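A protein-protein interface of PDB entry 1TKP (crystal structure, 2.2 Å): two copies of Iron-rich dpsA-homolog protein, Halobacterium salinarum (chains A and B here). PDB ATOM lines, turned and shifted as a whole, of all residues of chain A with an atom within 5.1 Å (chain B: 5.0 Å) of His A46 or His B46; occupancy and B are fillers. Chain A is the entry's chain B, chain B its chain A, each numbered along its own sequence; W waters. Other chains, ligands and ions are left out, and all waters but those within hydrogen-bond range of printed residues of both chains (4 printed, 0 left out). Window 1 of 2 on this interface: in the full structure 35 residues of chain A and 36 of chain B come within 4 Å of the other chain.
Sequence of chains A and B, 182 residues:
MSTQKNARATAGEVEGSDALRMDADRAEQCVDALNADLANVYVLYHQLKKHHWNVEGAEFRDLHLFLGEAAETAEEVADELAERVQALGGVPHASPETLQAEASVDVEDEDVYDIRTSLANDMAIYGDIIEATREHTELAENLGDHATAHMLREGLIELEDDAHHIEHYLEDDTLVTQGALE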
ATOM      1  N   TYR A  42      30.461  -1.363   4.206  1.00  0.00           N
ATOM      2  CA  TYR A  42      29.639  -0.882   5.275  1.00  0.00           C
ATOM      3  C   TYR A  42      29.028  -1.961   6.090  1.00  0.00           C
ATOM      4  O   TYR A  42      28.836  -1.757   7.232  1.00  0.00           O
ATOM      5  CB  TYR A  42      28.614   0.141   4.838  1.00  0.00           C
ATOM      6  CG  TYR A  42      28.925   1.507   5.407  1.00  0.00           C
ATOM      7  CD1 TYR A  42      28.831   2.633   4.622  1.00  0.00           C
ATOM      8  CD2 TYR A  42      29.271   1.682   6.776  1.00  0.00           C
ATOM      9  CE1 TYR A  42      29.123   3.873   5.092  1.00  0.00           C
ATOM     10  CE2 TYR A  42      29.596   2.972   7.277  1.00  0.00           C
ATOM     11  CZ  TYR A  42      29.482   4.032   6.370  1.00  0.00           C
ATOM     12  OH  TYR A  42      29.720   5.274   6.740  1.00  0.00           O
ATOM     13  N   VAL A  43      28.723  -3.152   5.556  1.00  0.00           N
ATOM     14  CA  VAL A  43      28.235  -4.237   6.427  1.00  0.00           C
ATOM     15  C   VAL A  43      29.421  -4.722   7.198  1.00  0.00           C
ATOM     16  O   VAL A  43      29.324  -4.885   8.390  1.00  0.00           O
ATOM     17  CB  VAL A  43      27.327  -5.387   5.771  1.00  0.00           C
ATOM     18  CG1 VAL A  43      26.320  -4.860   4.839  1.00  0.00           C
ATOM     19  CG2 VAL A  43      28.095  -6.388   5.153  1.00  0.00           C
ATOM     20  N   LEU A  44      30.583  -4.775   6.592  1.00  0.00           N
ATOM     21  CA  LEU A  44      31.744  -5.192   7.297  1.00  0.00           C
ATOM     22  C   LEU A  44      31.934  -4.257   8.539  1.00  0.00           C
ATOM     23  O   LEU A  44      32.135  -4.793   9.686  1.00  0.00           O
ATOM     24  CB  LEU A  44      32.971  -5.165   6.405  1.00  0.00           C
ATOM     25  CG  LEU A  44      34.315  -5.361   7.175  1.00  0.00           C
ATOM     26  CD1 LEU A  44      34.584  -6.806   7.738  1.00  0.00           C
ATOM     27  CD2 LEU A  44      35.453  -4.978   6.385  1.00  0.00           C
ATOM     28  N   TYR A  45      31.741  -2.941   8.351  1.00  0.00           N
ATOM     29  CA  TYR A  45      31.977  -1.997   9.414  1.00  0.00           C
ATOM     30  C   TYR A  45      31.012  -2.251  10.502  1.00  0.00           C
ATOM     31  O   TYR A  45      31.342  -2.192  11.650  1.00  0.00           O
ATOM     32  CB  TYR A  45      31.735  -0.603   8.900  1.00  0.00           C
ATOM     33  CG  TYR A  45      31.447   0.451   9.943  1.00  0.00           C
ATOM     34  CD1 TYR A  45      32.499   1.096  10.690  1.00  0.00           C
ATOM     35  CD2 TYR A  45      30.173   0.876  10.122  1.00  0.00           C
ATOM     36  CE1 TYR A  45      32.194   2.045  11.560  1.00  0.00           C
ATOM     37  CE2 TYR A  45      29.890   1.873  10.963  1.00  0.00           C
ATOM     38  CZ  TYR A  45      30.885   2.446  11.689  1.00  0.00           C
ATOM     39  OH  TYR A  45      30.439   3.366  12.583  1.00  0.00           O
ATOM     40  N   HIS A  46      29.794  -2.570  10.156  1.00  0.00           N
ATOM     41  CA  HIS A  46      28.757  -2.686  11.194  1.00  0.00           C
ATOM     42  C   HIS A  46      28.990  -4.026  11.926  1.00  0.00           C
ATOM     43  O   HIS A  46      28.804  -4.062  13.104  1.00  0.00           O
ATOM     44  CB  HIS A  46      27.314  -2.582  10.601  1.00  0.00           C
ATOM     45  CG  HIS A  46      26.770  -1.180  10.603  1.00  0.00           C
ATOM     46  ND1 HIS A  46      26.588  -0.458  11.762  1.00  0.00           N
ATOM     47  CD2 HIS A  46      26.487  -0.332   9.603  1.00  0.00           C
ATOM     48  CE1 HIS A  46      26.147   0.762  11.474  1.00  0.00           C
ATOM     49  NE2 HIS A  46      26.129   0.883  10.167  1.00  0.00           N
ATOM     50  N   GLN A  47      29.555  -5.025  11.272  1.00  0.00           N
ATOM     51  CA  GLN A  47      29.860  -6.288  11.956  1.00  0.00           C
ATOM     52  C   GLN A  47      31.159  -6.213  12.813  1.00  0.00           C
ATOM     53  O   GLN A  47      31.269  -6.837  13.849  1.00  0.00           O
ATOM     54  CB  GLN A  47      29.999  -7.424  10.995  1.00  0.00           C
ATOM     55  CG  GLN A  47      30.003  -8.776  11.713  1.00  0.00           C
ATOM     56  CD  GLN A  47      29.576  -9.886  10.792  1.00  0.00           C
ATOM     57  OE1 GLN A  47      28.389 -10.022  10.428  1.00  0.00           O
ATOM     58  NE2 GLN A  47      30.525 -10.726  10.438  1.00  0.00           N
ATOM     59  N   LEU A  48      32.081  -5.381  12.387  1.00  0.00           N
ATOM     60  CA  LEU A  48      33.225  -5.113  13.171  1.00  0.00           C
ATOM     61  C   LEU A  48      32.817  -4.352  14.428  1.00  0.00           C
ATOM     62  O   LEU A  48      33.375  -4.622  15.483  1.00  0.00           O
ATOM     63  CB  LEU A  48      34.261  -4.333  12.364  1.00  0.00           C
ATOM     64  CG  LEU A  48      34.930  -5.074  11.221  1.00  0.00           C
ATOM     65  CD1 LEU A  48      35.884  -4.156  10.405  1.00  0.00           C
ATOM     66  CD2 LEU A  48      35.649  -6.288  11.811  1.00  0.00           C
ATOM     67  N   LYS A  49      31.867  -3.420  14.298  1.00  0.00           N
ATOM     68  CA  LYS A  49      31.381  -2.660  15.422  1.00  0.00           C
ATOM     69  C   LYS A  49      30.767  -3.611  16.376  1.00  0.00           C
ATOM     70  O   LYS A  49      31.001  -3.551  17.604  1.00  0.00           O
ATOM     71  CB  LYS A  49      30.269  -1.678  15.021  1.00  0.00           C
ATOM     72  CG  LYS A  49      30.823  -0.359  14.379  1.00  0.00           C
ATOM     73  CD  LYS A  49      32.084   0.337  15.058  1.00  0.00           C
ATOM     74  CE  LYS A  49      31.774   0.785  16.437  1.00  0.00           C
ATOM     75  NZ  LYS A  49      32.416   2.241  16.705  1.00  0.00           N
ATOM     76  N   LYS A  50      29.990  -4.528  15.833  1.00  0.00           N
ATOM     77  CA  LYS A  50      29.345  -5.491  16.648  1.00  0.00           C
ATOM     78  C   LYS A  50      30.272  -6.351  17.506  1.00  0.00           C
ATOM     79  O   LYS A  50      30.022  -6.617  18.727  1.00  0.00           O
ATOM     80  CB  LYS A  50      28.512  -6.444  15.816  1.00  0.00           C
ATOM     81  CG  LYS A  50      27.845  -7.378  16.687  1.00  0.00           C
ATOM     82  CD  LYS A  50      27.014  -8.330  15.756  1.00  0.00           C
ATOM     83  CE  LYS A  50      26.482  -9.494  16.455  1.00  0.00           C
ATOM     84  NZ  LYS A  50      25.767 -10.588  15.539  1.00  0.00           N
ATOM     85  N   ALA A  94      23.118   4.466   0.538  1.00  0.00           N
ATOM     86  CA  ALA A  94      23.184   5.245   1.728  1.00  0.00           C
ATOM     87  C   ALA A  94      22.461   4.646   2.914  1.00  0.00           C
ATOM     88  O   ALA A  94      23.068   4.572   3.959  1.00  0.00           O
ATOM     89  CB  ALA A  94      22.717   6.693   1.485  1.00  0.00           C
ATOM     90  N   SER A  95      21.164   4.292   2.844  1.00  0.00           N
ATOM     91  CA  SER A  95      20.497   3.892   4.103  1.00  0.00           C
ATOM     92  C   SER A  95      21.048   2.594   4.548  1.00  0.00           C
ATOM     93  O   SER A  95      21.563   1.822   3.763  1.00  0.00           O
ATOM     94  CB  SER A  95      19.019   3.751   3.961  1.00  0.00           C
ATOM     95  OG  SER A  95      18.771   2.661   3.077  1.00  0.00           O
ATOM     96  N   PRO A  96      20.944   2.296   5.813  1.00  0.00           N
ATOM     97  CA  PRO A  96      21.420   0.984   6.300  1.00  0.00           C
ATOM     98  C   PRO A  96      20.780  -0.193   5.554  1.00  0.00           C
ATOM     99  O   PRO A  96      21.550  -1.100   5.130  1.00  0.00           O
ATOM    100  CB  PRO A  96      21.055   0.993   7.803  1.00  0.00           C
ATOM    101  CG  PRO A  96      21.153   2.611   8.114  1.00  0.00           C
ATOM    102  CD  PRO A  96      20.481   3.213   6.861  1.00  0.00           C
ATOM    103  N   LEU A  99      22.301  -0.563   2.229  1.00  0.00           N
ATOM    104  CA  LEU A  99      23.643  -1.106   2.268  1.00  0.00           C
ATOM    105  C   LEU A  99      23.623  -2.627   2.480  1.00  0.00           C
ATOM    106  O   LEU A  99      24.456  -3.394   1.900  1.00  0.00           O
ATOM    107  CB  LEU A  99      24.436  -0.396   3.409  1.00  0.00           C
ATOM    108  CG  LEU A  99      24.819   1.091   3.153  1.00  0.00           C
ATOM    109  CD1 LEU A  99      25.187   1.882   4.469  1.00  0.00           C
ATOM    110  CD2 LEU A  99      25.980   1.178   2.133  1.00  0.00           C
ATOM    111  N   TYR B  42      22.227   5.540  14.639  1.00  0.00           N
ATOM    112  CA  TYR B  42      22.871   4.983  13.501  1.00  0.00           C
ATOM    113  C   TYR B  42      22.099   5.225  12.187  1.00  0.00           C
ATOM    114  O   TYR B  42      22.738   5.330  11.121  1.00  0.00           O
ATOM    115  CB  TYR B  42      23.071   3.480  13.700  1.00  0.00           C
ATOM    116  CG  TYR B  42      24.518   3.156  13.838  1.00  0.00           C
ATOM    117  CD1 TYR B  42      24.965   2.292  14.845  1.00  0.00           C
ATOM    118  CD2 TYR B  42      25.447   3.825  13.058  1.00  0.00           C
ATOM    119  CE1 TYR B  42      26.325   2.062  15.003  1.00  0.00           C
ATOM    120  CE2 TYR B  42      26.811   3.641  13.231  1.00  0.00           C
ATOM    121  CZ  TYR B  42      27.225   2.722  14.205  1.00  0.00           C
ATOM    122  OH  TYR B  42      28.554   2.403  14.388  1.00  0.00           O
ATOM    123  N   VAL B  43      20.754   5.317  12.174  1.00  0.00           N
ATOM    124  CA  VAL B  43      20.233   5.802  10.901  1.00  0.00           C
ATOM    125  C   VAL B  43      20.544   7.298  10.673  1.00  0.00           C
ATOM    126  O   VAL B  43      20.845   7.750   9.533  1.00  0.00           O
ATOM    127  CB  VAL B  43      18.769   5.420  10.522  1.00  0.00           C
ATOM    128  CG1 VAL B  43      18.231   4.094  11.090  1.00  0.00           C
ATOM    129  CG2 VAL B  43      17.832   6.508  10.555  1.00  0.00           C
ATOM    130  N   LEU B  44      20.544   8.080  11.738  1.00  0.00           N
ATOM    131  CA  LEU B  44      20.957   9.445  11.580  1.00  0.00           C
ATOM    132  C   LEU B  44      22.363   9.480  10.946  1.00  0.00           C
ATOM    133  O   LEU B  44      22.611  10.217   9.997  1.00  0.00           O
ATOM    134  CB  LEU B  44      21.081  10.068  12.954  1.00  0.00           C
ATOM    135  CG  LEU B  44      21.626  11.496  12.932  1.00  0.00           C
ATOM    136  CD1 LEU B  44      20.814  12.410  11.997  1.00  0.00           C
ATOM    137  CD2 LEU B  44      21.721  12.151  14.317  1.00  0.00           C
ATOM    138  N   TYR B  45      23.270   8.661  11.487  1.00  0.00           N
ATOM    139  CA  TYR B  45      24.649   8.718  11.039  1.00  0.00           C
ATOM    140  C   TYR B  45      24.690   8.412   9.523  1.00  0.00           C
ATOM    141  O   TYR B  45      25.311   9.122   8.741  1.00  0.00           O
ATOM    142  CB  TYR B  45      25.505   7.734  11.881  1.00  0.00           C
ATOM    143  CG  TYR B  45      26.759   7.252  11.189  1.00  0.00           C
ATOM    144  CD1 TYR B  45      28.034   7.922  11.414  1.00  0.00           C
ATOM    145  CD2 TYR B  45      26.722   6.135  10.405  1.00  0.00           C
ATOM    146  CE1 TYR B  45      29.210   7.443  10.834  1.00  0.00           C
ATOM    147  CE2 TYR B  45      27.846   5.666   9.785  1.00  0.00           C
ATOM    148  CZ  TYR B  45      29.064   6.300  10.021  1.00  0.00           C
ATOM    149  OH  TYR B  45      30.136   5.837   9.366  1.00  0.00           O
ATOM    150  N   HIS B  46      23.996   7.367   9.093  1.00  0.00           N
ATOM    151  CA  HIS B  46      24.031   7.023   7.690  1.00  0.00           C
ATOM    152  C   HIS B  46      23.431   8.114   6.821  1.00  0.00           C
ATOM    153  O   HIS B  46      23.937   8.384   5.787  1.00  0.00           O
ATOM    154  CB  HIS B  46      23.388   5.688   7.460  1.00  0.00           C
ATOM    155  CG  HIS B  46      24.335   4.513   7.634  1.00  0.00           C
ATOM    156  ND1 HIS B  46      25.380   4.264   6.770  1.00  0.00           N
ATOM    157  CD2 HIS B  46      24.349   3.525   8.536  1.00  0.00           C
ATOM    158  CE1 HIS B  46      26.058   3.210   7.202  1.00  0.00           C
ATOM    159  NE2 HIS B  46      25.428   2.727   8.251  1.00  0.00           N
ATOM    160  N   GLN B  47      22.395   8.815   7.270  1.00  0.00           N
ATOM    161  CA  GLN B  47      21.807   9.866   6.464  1.00  0.00           C
ATOM    162  C   GLN B  47      22.730  11.094   6.422  1.00  0.00           C
ATOM    163  O   GLN B  47      22.877  11.749   5.361  1.00  0.00           O
ATOM    164  CB  GLN B  47      20.437  10.270   6.991  1.00  0.00           C
ATOM    165  CG  GLN B  47      19.734  11.183   5.996  1.00  0.00           C
ATOM    166  CD  GLN B  47      18.231  10.943   6.046  1.00  0.00           C
ATOM    167  OE1 GLN B  47      17.802   9.855   5.648  1.00  0.00           O
ATOM    168  NE2 GLN B  47      17.453  11.890   6.647  1.00  0.00           N
ATOM    169  N   LEU B  48      23.386  11.398   7.509  1.00  0.00           N
ATOM    170  CA  LEU B  48      24.379  12.486   7.496  1.00  0.00           C
ATOM    171  C   LEU B  48      25.515  12.197   6.606  1.00  0.00           C
ATOM    172  O   LEU B  48      25.988  13.027   5.831  1.00  0.00           O
ATOM    173  CB  LEU B  48      24.933  12.656   8.871  1.00  0.00           C
ATOM    174  CG  LEU B  48      23.915  13.172   9.889  1.00  0.00           C
ATOM    175  CD1 LEU B  48      24.437  13.116  11.254  1.00  0.00           C
ATOM    176  CD2 LEU B  48      23.426  14.645   9.564  1.00  0.00           C
ATOM    177  N   LYS B  49      26.029  11.002   6.687  1.00  0.00           N
ATOM    178  CA  LYS B  49      27.021  10.582   5.680  1.00  0.00           C
ATOM    179  C   LYS B  49      26.478  10.826   4.266  1.00  0.00           C
ATOM    180  O   LYS B  49      27.116  11.402   3.384  1.00  0.00           O
ATOM    181  CB  LYS B  49      27.346   9.105   5.844  1.00  0.00           C
ATOM    182  CG  LYS B  49      28.170   8.718   7.021  1.00  0.00           C
ATOM    183  CD  LYS B  49      29.431   9.474   7.181  1.00  0.00           C
ATOM    184  CE  LYS B  49      30.472   9.145   6.264  1.00  0.00           C
ATOM    185  NZ  LYS B  49      31.911   9.370   6.947  1.00  0.00           N
ATOM    186  N   LYS B  50      25.292  10.369   4.053  1.00  0.00           N
ATOM    187  CA  LYS B  50      24.678  10.464   2.689  1.00  0.00           C
ATOM    188  C   LYS B  50      24.755  11.962   2.244  1.00  0.00           C
ATOM    189  O   LYS B  50      25.185  12.301   1.098  1.00  0.00           O
ATOM    190  CB  LYS B  50      23.223  10.041   2.751  1.00  0.00           C
ATOM    191  CG  LYS B  50      22.501  10.306   1.414  1.00  0.00           C
ATOM    192  CD  LYS B  50      21.028  10.209   1.474  1.00  0.00           C
ATOM    193  CE  LYS B  50      20.535  10.009  -0.041  1.00  0.00           C
ATOM    194  NZ  LYS B  50      19.122   9.564  -0.036  1.00  0.00           N
ATOM    195  N   ALA B  94      22.825  -4.460  15.758  1.00  0.00           N
ATOM    196  CA  ALA B  94      24.108  -4.497  15.090  1.00  0.00           C
ATOM    197  C   ALA B  94      23.993  -4.388  13.555  1.00  0.00           C
ATOM    198  O   ALA B  94      24.546  -3.453  12.996  1.00  0.00           O
ATOM    199  CB  ALA B  94      24.879  -5.775  15.498  1.00  0.00           C
ATOM    200  N   SER B  95      23.294  -5.291  12.889  1.00  0.00           N
ATOM    201  CA  SER B  95      23.344  -5.312  11.440  1.00  0.00           C
ATOM    202  C   SER B  95      22.631  -4.097  10.932  1.00  0.00           C
ATOM    203  O   SER B  95      21.858  -3.512  11.648  1.00  0.00           O
ATOM    204  CB  SER B  95      22.659  -6.567  10.882  1.00  0.00           C
ATOM    205  OG  SER B  95      21.260  -6.404  11.169  1.00  0.00           O
ATOM    206  N   PRO B  96      22.991  -3.612   9.772  1.00  0.00           N
ATOM    207  CA  PRO B  96      22.333  -2.421   9.239  1.00  0.00           C
ATOM    208  C   PRO B  96      20.804  -2.599   9.092  1.00  0.00           C
ATOM    209  O   PRO B  96      19.946  -1.718   9.344  1.00  0.00           O
ATOM    210  CB  PRO B  96      23.026  -2.264   7.895  1.00  0.00           C
ATOM    211  CG  PRO B  96      24.413  -2.662   8.225  1.00  0.00           C
ATOM    212  CD  PRO B  96      24.198  -3.969   8.986  1.00  0.00           C
ATOM    213  N   LEU B  99      19.257  -2.268  12.469  1.00  0.00           N
ATOM    214  CA  LEU B  99      19.277  -0.931  12.955  1.00  0.00           C
ATOM    215  C   LEU B  99      18.187  -0.100  12.314  1.00  0.00           C
ATOM    216  O   LEU B  99      17.477   0.580  13.015  1.00  0.00           O
ATOM    217  CB  LEU B  99      20.665  -0.310  12.716  1.00  0.00           C
ATOM    218  CG  LEU B  99      21.788  -0.711  13.656  1.00  0.00           C
ATOM    219  CD1 LEU B  99      23.143  -0.251  13.116  1.00  0.00           C
ATOM    220  CD2 LEU B  99      21.568  -0.069  15.019  1.00  0.00           C
HETATM  221  O   HOH W   1      32.195   6.525   5.867  1.00  0.00           O
HETATM  222  O   HOH W   2      29.679   3.674  16.625  1.00  0.00           O
HETATM  223  O   HOH W   3      25.252   5.753   4.696  1.00  0.00           O
HETATM  224  O   HOH W   4      26.678  -2.253  13.897  1.00  0.00           O
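Water W3 lies within hydrogen-bond range of a ring nitrogen (ND1) of His B46 (2.6 Å) and the backbone carbonyl oxygen (O) of Ala A94 (2.6 Å).
Water W4 lies within hydrogen-bond range of the backbone carbonyl oxygen of Ala B94 (2.6 Å) and a ring nitrogen (ND1) of His A46 (2.8 Å).
Water W2 lies within hydrogen-bond range of OH of Tyr B42 and NZ of Lys A49.
Water W1 lies within hydrogen-bond range of the side-chain hydroxyl of Tyr A42 (2.9 Å) and the side-chain amino group of Lys B49 (3.1 Å).
OH of Tyr B42 sits at hydrogen-bond distance from OH of Tyr A45 (2.8 Å).
The side-chain hydroxyl (OH) of Tyr B45 is in hydrogen-bond range of the side-chain hydroxyl (OH) of Tyr A42, at 2.7 Å.
NE2 of His B46 lies within hydrogen-bond range of NE2 of His A46, 2.8 Å away.
Of the 13 printed residues of chain A, 8 touch a printed residue of chain B.
Hydrophobic or aromatic side chains of chain A that line the printed part of chain B: Tyr A42, Tyr A45, His A46, Ala A94, Pro A96 and Leu A99.
Hydrophobic or aromatic side chains of chain B that line the printed part of chain A: Tyr B42, Tyr B45, His B46, Ala B94, Pro B96 and Leu B99.
Among the printed residues, no Asp or Glu carboxylate lies within 4 Å of a Lys or Arg side-chain nitrogen of the other chain.
Tyr A42 touches His B46, and with the chains exchanged His A46 touches Tyr B42.
Tyr A42 touches Lys B49, and with the chains exchanged Lys A49 touches Tyr B42.
His A46 touches Leu B99, and with the chains exchanged Leu A99 touches His B46.
Lys A50 touches Ala B94, and with the chains exchanged Ala A94 touches Lys B50.
Of the 16 pairs that touch across the chains among the printed residues, 16 have their exchanged pair printed and touching as well.
His A46 touches five residues of chain B.
Printed residues of chain B within 4 Å of Pro A96: His B46 (3.4 Å) and Pro B96 (3.3 Å).
His B46 touches just these residues of chain A: Tyr A42 (3.5 Å), His A46 (2.8 Å), Ala A94 (3.7 Å), Pro A96 (3.4 Å) and Leu A99 (3.2 Å).
Printed residues of chain A within 4 Å of Lys B50: Ala A94.
The nearest residue of chain B that does not touch His A46 is Ser B95 (4.9 Å).
Among the printed residues, merely in contact across the chains: Leu A99 with His B46 (3.2 Å), Pro A96 with Pro B96 (3.3 Å), Lys A50 with Ala B94 (3.3 Å), Pro A96 with His B46 (3.4 Å), His A46 with Pro B96 (3.4 Å), His A46 with Tyr B42 (3.4 Å), Tyr A42 with His B46 (3.5 Å), His A46 with Leu B99 (3.6 Å), Lys A49 with Tyr B42 (3.6 Å), Ala A94 with Lys B50 (3.6 Å), Ala A94 with His B46 (3.7 Å), His A46 with Ala B94 (3.8 Å) and Tyr A42 with Lys B49 (3.8 Å).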
